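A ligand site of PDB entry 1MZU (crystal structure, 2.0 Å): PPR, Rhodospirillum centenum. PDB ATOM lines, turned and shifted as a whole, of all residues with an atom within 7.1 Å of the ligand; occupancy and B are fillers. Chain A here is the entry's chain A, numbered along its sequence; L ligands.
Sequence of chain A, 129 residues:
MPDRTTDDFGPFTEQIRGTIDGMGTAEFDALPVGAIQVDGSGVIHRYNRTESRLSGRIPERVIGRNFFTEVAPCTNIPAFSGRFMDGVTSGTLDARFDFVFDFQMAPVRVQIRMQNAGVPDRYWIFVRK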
ATOM      1  N   ILE A  36     -12.178  12.905  12.835  1.00  0.00           N
ATOM      2  CA  ILE A  36     -12.456  14.135  13.583  1.00  0.00           C
ATOM      3  C   ILE A  36     -11.247  14.577  14.405  1.00  0.00           C
ATOM      4  O   ILE A  36     -10.681  13.754  15.137  1.00  0.00           O
ATOM      5  CB  ILE A  36     -13.643  13.963  14.592  1.00  0.00           C
ATOM      6  CG1 ILE A  36     -14.882  13.406  13.885  1.00  0.00           C
ATOM      7  CG2 ILE A  36     -13.989  15.307  15.269  1.00  0.00           C
ATOM      8  CD1 ILE A  36     -15.790  12.554  14.745  1.00  0.00           C
ATOM      9  N   ILE A  44     -14.023  20.794  18.270  1.00  0.00           N
ATOM     10  CA  ILE A  44     -13.761  20.307  16.902  1.00  0.00           C
ATOM     11  C   ILE A  44     -13.027  21.316  16.007  1.00  0.00           C
ATOM     12  O   ILE A  44     -13.440  22.471  15.869  1.00  0.00           O
ATOM     13  CB  ILE A  44     -15.081  19.808  16.223  1.00  0.00           C
ATOM     14  CG1 ILE A  44     -15.694  18.702  17.091  1.00  0.00           C
ATOM     15  CG2 ILE A  44     -14.807  19.284  14.779  1.00  0.00           C
ATOM     16  CD1 ILE A  44     -17.056  18.251  16.704  1.00  0.00           C
ATOM     17  N   TYR A  47     -13.289  18.091  10.551  1.00  0.00           N
ATOM     18  CA  TYR A  47     -14.414  17.148  10.458  1.00  0.00           C
ATOM     19  C   TYR A  47     -14.575  16.773   8.976  1.00  0.00           C
ATOM     20  O   TYR A  47     -15.024  17.607   8.176  1.00  0.00           O
ATOM     21  CB  TYR A  47     -15.685  17.852  10.972  1.00  0.00           C
ATOM     22  CG  TYR A  47     -16.870  16.968  11.293  1.00  0.00           C
ATOM     23  CD1 TYR A  47     -17.007  16.368  12.558  1.00  0.00           C
ATOM     24  CD2 TYR A  47     -17.866  16.719  10.321  1.00  0.00           C
ATOM     25  CE1 TYR A  47     -18.122  15.527  12.862  1.00  0.00           C
ATOM     26  CE2 TYR A  47     -18.976  15.894  10.610  1.00  0.00           C
ATOM     27  CZ  TYR A  47     -19.100  15.296  11.870  1.00  0.00           C
ATOM     28  OH  TYR A  47     -20.157  14.455  12.092  1.00  0.00           O
ATOM     29  N   GLU A  51     -17.392  11.108   7.636  1.00  0.00           N
ATOM     30  CA  GLU A  51     -18.028  11.172   8.949  1.00  0.00           C
ATOM     31  C   GLU A  51     -19.370  11.887   8.841  1.00  0.00           C
ATOM     32  O   GLU A  51     -20.311  11.523   9.530  1.00  0.00           O
ATOM     33  CB  GLU A  51     -17.129  11.882   9.974  1.00  0.00           C
ATOM     34  CG  GLU A  51     -17.588  11.794  11.470  1.00  0.00           C
ATOM     35  CD  GLU A  51     -17.835  10.366  11.990  1.00  0.00           C
ATOM     36  OE1 GLU A  51     -17.313   9.379  11.423  1.00  0.00           O
ATOM     37  OE2 GLU A  51     -18.558  10.238  13.004  1.00  0.00           O
ATOM     38  N   SER A  52     -19.409  12.895   7.963  1.00  0.00           N
ATOM     39  CA  SER A  52     -20.620  13.666   7.686  1.00  0.00           C
ATOM     40  C   SER A  52     -21.673  12.761   7.051  1.00  0.00           C
ATOM     41  O   SER A  52     -22.849  12.890   7.347  1.00  0.00           O
ATOM     42  CB  SER A  52     -20.314  14.820   6.731  1.00  0.00           C
ATOM     43  OG  SER A  52     -21.492  15.503   6.345  1.00  0.00           O
ATOM     44  N   LEU A  54     -21.872   9.469   7.499  1.00  0.00           N
ATOM     45  CA  LEU A  54     -22.285   8.519   8.513  1.00  0.00           C
ATOM     46  C   LEU A  54     -23.154   9.160   9.597  1.00  0.00           C
ATOM     47  O   LEU A  54     -23.993   8.493  10.201  1.00  0.00           O
ATOM     48  CB  LEU A  54     -21.072   7.841   9.181  1.00  0.00           C
ATOM     49  CG  LEU A  54     -20.166   6.869   8.403  1.00  0.00           C
ATOM     50  CD1 LEU A  54     -19.123   6.267   9.341  1.00  0.00           C
ATOM     51  CD2 LEU A  54     -20.982   5.752   7.761  1.00  0.00           C
ATOM     52  N   SER A  55     -23.005  10.472   9.784  1.00  0.00           N
ATOM     53  CA  SER A  55     -23.737  11.205  10.813  1.00  0.00           C
ATOM     54  C   SER A  55     -24.898  12.081  10.390  1.00  0.00           C
ATOM     55  O   SER A  55     -25.847  12.260  11.159  1.00  0.00           O
ATOM     56  CB  SER A  55     -22.762  12.068  11.618  1.00  0.00           C
ATOM     57  OG  SER A  55     -22.364  13.226  10.897  1.00  0.00           O
ATOM     58  N   GLY A  56     -24.769  12.702   9.218  1.00  0.00           N
ATOM     59  CA  GLY A  56     -25.802  13.589   8.697  1.00  0.00           C
ATOM     60  C   GLY A  56     -25.509  15.040   9.071  1.00  0.00           C
ATOM     61  O   GLY A  56     -26.298  15.936   8.769  1.00  0.00           O
ATOM     62  N   ARG A  57     -24.378  15.259   9.753  1.00  0.00           N
ATOM     63  CA  ARG A  57     -23.950  16.595  10.187  1.00  0.00           C
ATOM     64  C   ARG A  57     -23.104  17.302   9.143  1.00  0.00           C
ATOM     65  O   ARG A  57     -22.233  16.702   8.542  1.00  0.00           O
ATOM     66  CB  ARG A  57     -23.147  16.529  11.492  1.00  0.00           C
ATOM     67  CG  ARG A  57     -23.966  16.544  12.782  1.00  0.00           C
ATOM     68  CD  ARG A  57     -24.581  15.193  13.083  1.00  0.00           C
ATOM     69  NE  ARG A  57     -25.255  15.167  14.373  1.00  0.00           N
ATOM     70  CZ  ARG A  57     -26.079  14.200  14.774  1.00  0.00           C
ATOM     71  NH1 ARG A  57     -26.338  13.165  13.981  1.00  0.00           N
ATOM     72  NH2 ARG A  57     -26.654  14.267  15.964  1.00  0.00           N
ATOM     73  N   VAL A  62     -20.609  22.373  12.770  1.00  0.00           N
ATOM     74  CA  VAL A  62     -20.027  21.472  13.769  1.00  0.00           C
ATOM     75  C   VAL A  62     -18.617  21.911  14.235  1.00  0.00           C
ATOM     76  O   VAL A  62     -18.266  21.711  15.396  1.00  0.00           O
ATOM     77  CB  VAL A  62     -20.085  20.001  13.223  1.00  0.00           C
ATOM     78  CG1 VAL A  62     -19.247  19.053  14.013  1.00  0.00           C
ATOM     79  CG2 VAL A  62     -21.518  19.514  13.278  1.00  0.00           C
ATOM     80  N   PHE A  67     -17.248  18.397  20.860  1.00  0.00           N
ATOM     81  CA  PHE A  67     -17.653  17.054  20.454  1.00  0.00           C
ATOM     82  C   PHE A  67     -18.421  16.306  21.543  1.00  0.00           C
ATOM     83  O   PHE A  67     -19.464  15.737  21.266  1.00  0.00           O
ATOM     84  CB  PHE A  67     -16.414  16.213  20.025  1.00  0.00           C
ATOM     85  CG  PHE A  67     -16.742  14.838  19.477  1.00  0.00           C
ATOM     86  CD1 PHE A  67     -17.382  14.688  18.227  1.00  0.00           C
ATOM     87  CD2 PHE A  67     -16.428  13.690  20.208  1.00  0.00           C
ATOM     88  CE1 PHE A  67     -17.710  13.394  17.720  1.00  0.00           C
ATOM     89  CE2 PHE A  67     -16.752  12.371  19.716  1.00  0.00           C
ATOM     90  CZ  PHE A  67     -17.392  12.239  18.472  1.00  0.00           C
ATOM     91  N   GLU A  70     -21.579  19.071  23.274  1.00  0.00           N
ATOM     92  CA  GLU A  70     -22.553  19.593  22.308  1.00  0.00           C
ATOM     93  C   GLU A  70     -22.944  18.738  21.101  1.00  0.00           C
ATOM     94  O   GLU A  70     -24.124  18.415  20.944  1.00  0.00           O
ATOM     95  CB  GLU A  70     -22.110  20.990  21.798  1.00  0.00           C
ATOM     96  CG  GLU A  70     -21.949  22.054  22.892  1.00  0.00           C
ATOM     97  CD  GLU A  70     -21.286  23.334  22.404  1.00  0.00           C
ATOM     98  OE1 GLU A  70     -20.114  23.284  21.967  1.00  0.00           O
ATOM     99  OE2 GLU A  70     -21.935  24.395  22.464  1.00  0.00           O
ATOM    100  N   VAL A  71     -21.969  18.351  20.266  1.00  0.00           N
ATOM    101  CA  VAL A  71     -22.239  17.563  19.045  1.00  0.00           C
ATOM    102  C   VAL A  71     -22.571  16.098  19.244  1.00  0.00           C
ATOM    103  O   VAL A  71     -23.515  15.595  18.635  1.00  0.00           O
ATOM    104  CB  VAL A  71     -21.052  17.654  17.996  1.00  0.00           C
ATOM    105  CG1 VAL A  71     -21.458  17.011  16.659  1.00  0.00           C
ATOM    106  CG2 VAL A  71     -20.677  19.103  17.761  1.00  0.00           C
ATOM    107  N   ALA A  72     -21.839  15.417  20.128  1.00  0.00           N
ATOM    108  CA  ALA A  72     -22.061  13.996  20.346  1.00  0.00           C
ATOM    109  C   ALA A  72     -22.186  13.591  21.820  1.00  0.00           C
ATOM    110  O   ALA A  72     -21.332  12.865  22.327  1.00  0.00           O
ATOM    111  CB  ALA A  72     -20.922  13.206  19.679  1.00  0.00           C
ATOM    112  N   PRO A  73     -23.297  13.991  22.491  1.00  0.00           N
ATOM    113  CA  PRO A  73     -23.525  13.663  23.902  1.00  0.00           C
ATOM    114  C   PRO A  73     -23.539  12.193  24.318  1.00  0.00           C
ATOM    115  O   PRO A  73     -23.194  11.882  25.459  1.00  0.00           O
ATOM    116  CB  PRO A  73     -24.853  14.359  24.205  1.00  0.00           C
ATOM    117  CG  PRO A  73     -25.533  14.340  22.899  1.00  0.00           C
ATOM    118  CD  PRO A  73     -24.447  14.755  21.964  1.00  0.00           C
ATOM    119  N   CYS A  74     -23.885  11.292  23.388  1.00  0.00           N
ATOM    120  CA  CYS A  74     -23.912   9.840  23.650  1.00  0.00           C
ATOM    121  C   CYS A  74     -22.528   9.260  23.964  1.00  0.00           C
ATOM    122  O   CYS A  74     -22.404   8.139  24.441  1.00  0.00           O
ATOM    123  CB  CYS A  74     -24.654   9.079  22.559  1.00  0.00           C
ATOM    124  SG  CYS A  74     -23.735   8.872  20.978  1.00  0.00           S
ATOM    125  N   THR A  75     -21.491  10.031  23.632  1.00  0.00           N
ATOM    126  CA  THR A  75     -20.104   9.638  23.892  1.00  0.00           C
ATOM    127  C   THR A  75     -19.640  10.076  25.287  1.00  0.00           C
ATOM    128  O   THR A  75     -18.548   9.702  25.710  1.00  0.00           O
ATOM    129  CB  THR A  75     -19.135  10.269  22.851  1.00  0.00           C
ATOM    130  OG1 THR A  75     -19.050  11.688  23.054  1.00  0.00           O
ATOM    131  CG2 THR A  75     -19.584   9.970  21.423  1.00  0.00           C
ATOM    132  N   ASN A  76     -20.470  10.841  26.005  1.00  0.00           N
ATOM    133  CA  ASN A  76     -20.118  11.356  27.333  1.00  0.00           C
ATOM    134  C   ASN A  76     -20.207  10.367  28.509  1.00  0.00           C
ATOM    135  O   ASN A  76     -20.651  10.704  29.617  1.00  0.00           O
ATOM    136  CB  ASN A  76     -20.895  12.661  27.617  1.00  0.00           C
ATOM    137  CG  ASN A  76     -20.050  13.716  28.324  1.00  0.00           C
ATOM    138  OD1 ASN A  76     -20.565  14.503  29.112  1.00  0.00           O
ATOM    139  ND2 ASN A  76     -18.752  13.745  28.026  1.00  0.00           N
ATOM    140  N   PHE A  80     -15.979   6.245  26.497  1.00  0.00           N
ATOM    141  CA  PHE A  80     -15.550   7.119  25.395  1.00  0.00           C
ATOM    142  C   PHE A  80     -14.898   8.414  25.878  1.00  0.00           C
ATOM    143  O   PHE A  80     -13.707   8.597  25.632  1.00  0.00           O
ATOM    144  CB  PHE A  80     -16.747   7.397  24.444  1.00  0.00           C
ATOM    145  CG  PHE A  80     -16.359   7.708  22.993  1.00  0.00           C
ATOM    146  CD1 PHE A  80     -15.366   8.667  22.657  1.00  0.00           C
ATOM    147  CD2 PHE A  80     -17.075   7.117  21.937  1.00  0.00           C
ATOM    148  CE1 PHE A  80     -15.100   9.025  21.292  1.00  0.00           C
ATOM    149  CE2 PHE A  80     -16.831   7.472  20.576  1.00  0.00           C
ATOM    150  CZ  PHE A  80     -15.836   8.433  20.264  1.00  0.00           C
ATOM    151  N   PHE A  99     -18.124   0.514  19.598  1.00  0.00           N
ATOM    152  CA  PHE A  99     -19.135   1.448  20.082  1.00  0.00           C
ATOM    153  C   PHE A  99     -20.347   1.454  19.151  1.00  0.00           C
ATOM    154  O   PHE A  99     -20.277   0.991  18.017  1.00  0.00           O
ATOM    155  CB  PHE A  99     -18.538   2.861  20.132  1.00  0.00           C
ATOM    156  CG  PHE A  99     -19.149   3.742  21.188  1.00  0.00           C
ATOM    157  CD1 PHE A  99     -18.858   3.528  22.536  1.00  0.00           C
ATOM    158  CD2 PHE A  99     -20.051   4.775  20.831  1.00  0.00           C
ATOM    159  CE1 PHE A  99     -19.464   4.311  23.537  1.00  0.00           C
ATOM    160  CE2 PHE A  99     -20.664   5.561  21.820  1.00  0.00           C
ATOM    161  CZ  PHE A  99     -20.379   5.331  23.182  1.00  0.00           C
ATOM    162  N   VAL A 100     -21.452   2.014  19.659  1.00  0.00           N
ATOM    163  CA  VAL A 100     -22.685   2.110  18.899  1.00  0.00           C
ATOM    164  C   VAL A 100     -23.244   3.540  19.044  1.00  0.00           C
ATOM    165  O   VAL A 100     -23.382   4.056  20.163  1.00  0.00           O
ATOM    166  CB  VAL A 100     -23.721   0.993  19.320  1.00  0.00           C
ATOM    167  CG1 VAL A 100     -24.190   1.139  20.774  1.00  0.00           C
ATOM    168  CG2 VAL A 100     -24.897   0.944  18.370  1.00  0.00           C
ATOM    169  N   PHE A 101     -23.430   4.201  17.903  1.00  0.00           N
ATOM    170  CA  PHE A 101     -23.960   5.561  17.855  1.00  0.00           C
ATOM    171  C   PHE A 101     -25.488   5.559  17.796  1.00  0.00           C
ATOM    172  O   PHE A 101     -26.093   5.023  16.854  1.00  0.00           O
ATOM    173  CB  PHE A 101     -23.367   6.331  16.659  1.00  0.00           C
ATOM    174  CG  PHE A 101     -21.978   6.853  16.902  1.00  0.00           C
ATOM    175  CD1 PHE A 101     -21.549   7.183  18.201  1.00  0.00           C
ATOM    176  CD2 PHE A 101     -21.076   7.025  15.830  1.00  0.00           C
ATOM    177  CE1 PHE A 101     -20.245   7.666  18.446  1.00  0.00           C
ATOM    178  CE2 PHE A 101     -19.754   7.517  16.051  1.00  0.00           C
ATOM    179  CZ  PHE A 101     -19.346   7.834  17.383  1.00  0.00           C
ATOM    180  N   ASP A 102     -26.104   6.178  18.813  1.00  0.00           N
ATOM    181  CA  ASP A 102     -27.558   6.262  18.955  1.00  0.00           C
ATOM    182  C   ASP A 102     -28.170   7.488  18.273  1.00  0.00           C
ATOM    183  O   ASP A 102     -28.486   8.506  18.922  1.00  0.00           O
ATOM    184  CB  ASP A 102     -27.948   6.235  20.440  1.00  0.00           C
ATOM    185  CG  ASP A 102     -29.392   5.828  20.666  1.00  0.00           C
ATOM    186  OD1 ASP A 102     -29.817   4.782  20.125  1.00  0.00           O
ATOM    187  OD2 ASP A 102     -30.100   6.568  21.394  1.00  0.00           O
ATOM    188  N   PHE A 103     -28.357   7.361  16.961  1.00  0.00           N
ATOM    189  CA  PHE A 103     -28.928   8.426  16.136  1.00  0.00           C
ATOM    190  C   PHE A 103     -30.459   8.410  16.216  1.00  0.00           C
ATOM    191  O   PHE A 103     -31.036   7.546  16.870  1.00  0.00           O
ATOM    192  CB  PHE A 103     -28.458   8.280  14.682  1.00  0.00           C
ATOM    193  CG  PHE A 103     -26.977   8.521  14.487  1.00  0.00           C
ATOM    194  CD1 PHE A 103     -26.298   7.968  13.382  1.00  0.00           C
ATOM    195  CD2 PHE A 103     -26.256   9.333  15.389  1.00  0.00           C
ATOM    196  CE1 PHE A 103     -24.900   8.215  13.184  1.00  0.00           C
ATOM    197  CE2 PHE A 103     -24.884   9.592  15.209  1.00  0.00           C
ATOM    198  CZ  PHE A 103     -24.196   9.039  14.107  1.00  0.00           C
ATOM    199  N   VAL A 127     -13.360   6.753  12.919  1.00  0.00           N
ATOM    200  CA  VAL A 127     -14.608   5.979  13.023  1.00  0.00           C
ATOM    201  C   VAL A 127     -14.776   5.020  11.832  1.00  0.00           C
ATOM    202  O   VAL A 127     -14.787   5.455  10.680  1.00  0.00           O
ATOM    203  CB  VAL A 127     -15.826   6.986  13.051  1.00  0.00           C
ATOM    204  CG1 VAL A 127     -17.148   6.267  13.194  1.00  0.00           C
ATOM    205  CG2 VAL A 127     -15.687   8.007  14.177  1.00  0.00           C
HETATM  206  C1  LIG L   1     -24.011  10.379  20.098  1.00  0.00           C
HETATM  207  O1  LIG L   1     -24.656  11.370  20.593  1.00  0.00           O
HETATM  208  C2  LIG L   1     -23.316  10.407  18.839  1.00  0.00           C
HETATM  209  C3  LIG L   1     -23.407  11.422  17.990  1.00  0.00           C
HETATM  210  C4  LIG L   1     -22.531  11.658  16.876  1.00  0.00           C
HETATM  211  C5  LIG L   1     -22.759  12.847  16.044  1.00  0.00           C
HETATM  212  C6  LIG L   1     -21.860  13.148  14.995  1.00  0.00           C
HETATM  213  C7  LIG L   1     -20.708  12.329  14.801  1.00  0.00           C
HETATM  214  C8  LIG L   1     -20.493  11.188  15.612  1.00  0.00           C
HETATM  215  C9  LIG L   1     -21.385  10.884  16.640  1.00  0.00           C
HETATM  216  O2  LIG L   1     -19.848  12.589  13.835  1.00  0.00           O
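The backbone NH (N) of Cys 74 is in hydrogen-bond range of an oxygen (O1) of the ligand, at 2.9 Å.
O2 of the ligand is in hydrogen-bond range of OE2 of Glu 51 (2.8 Å).
The side-chain sulfur of Cys 74 is covalently linked to a carbon (C1) of the ligand (1.8 Å).
An oxygen (O2) of the ligand is in hydrogen-bond range of the side-chain hydroxyl (OH) of Tyr 47, 2.6 Å away.
OG of Ser 55 sits at hydrogen-bond distance from O of Glu 51 (3.0 Å).
The backbone carbonyl oxygen of Ala 72 is in hydrogen-bond range of the side-chain hydroxyl of Thr 75.
O of Ser 55 lies within hydrogen-bond range of NH1 of Arg 57 (3.0 Å).
O of Arg 57 sits at hydrogen-bond distance from OG of Ser 52 (2.6 Å).
OH of Tyr 47 lies within hydrogen-bond range of OG of Ser 55 (2.8 Å).
The backbone NH (N) of Ala 72 sits at hydrogen-bond distance from the backbone carbonyl oxygen (O) of Phe 67.
Residues that only touch the ligand: Ser 55, Arg 57, Val 71, Ala 72, Pro 73, Phe 101 and Phe 103.
Within 4 Å of the ligand: Tyr 47, Glu 51, Ser 55, Arg 57, Val 71, Ala 72, Pro 73, Cys 74, Phe 101 and Phe 103.
The nearest printed residue that does not touch the ligand is Phe 67 (4.1 Å).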
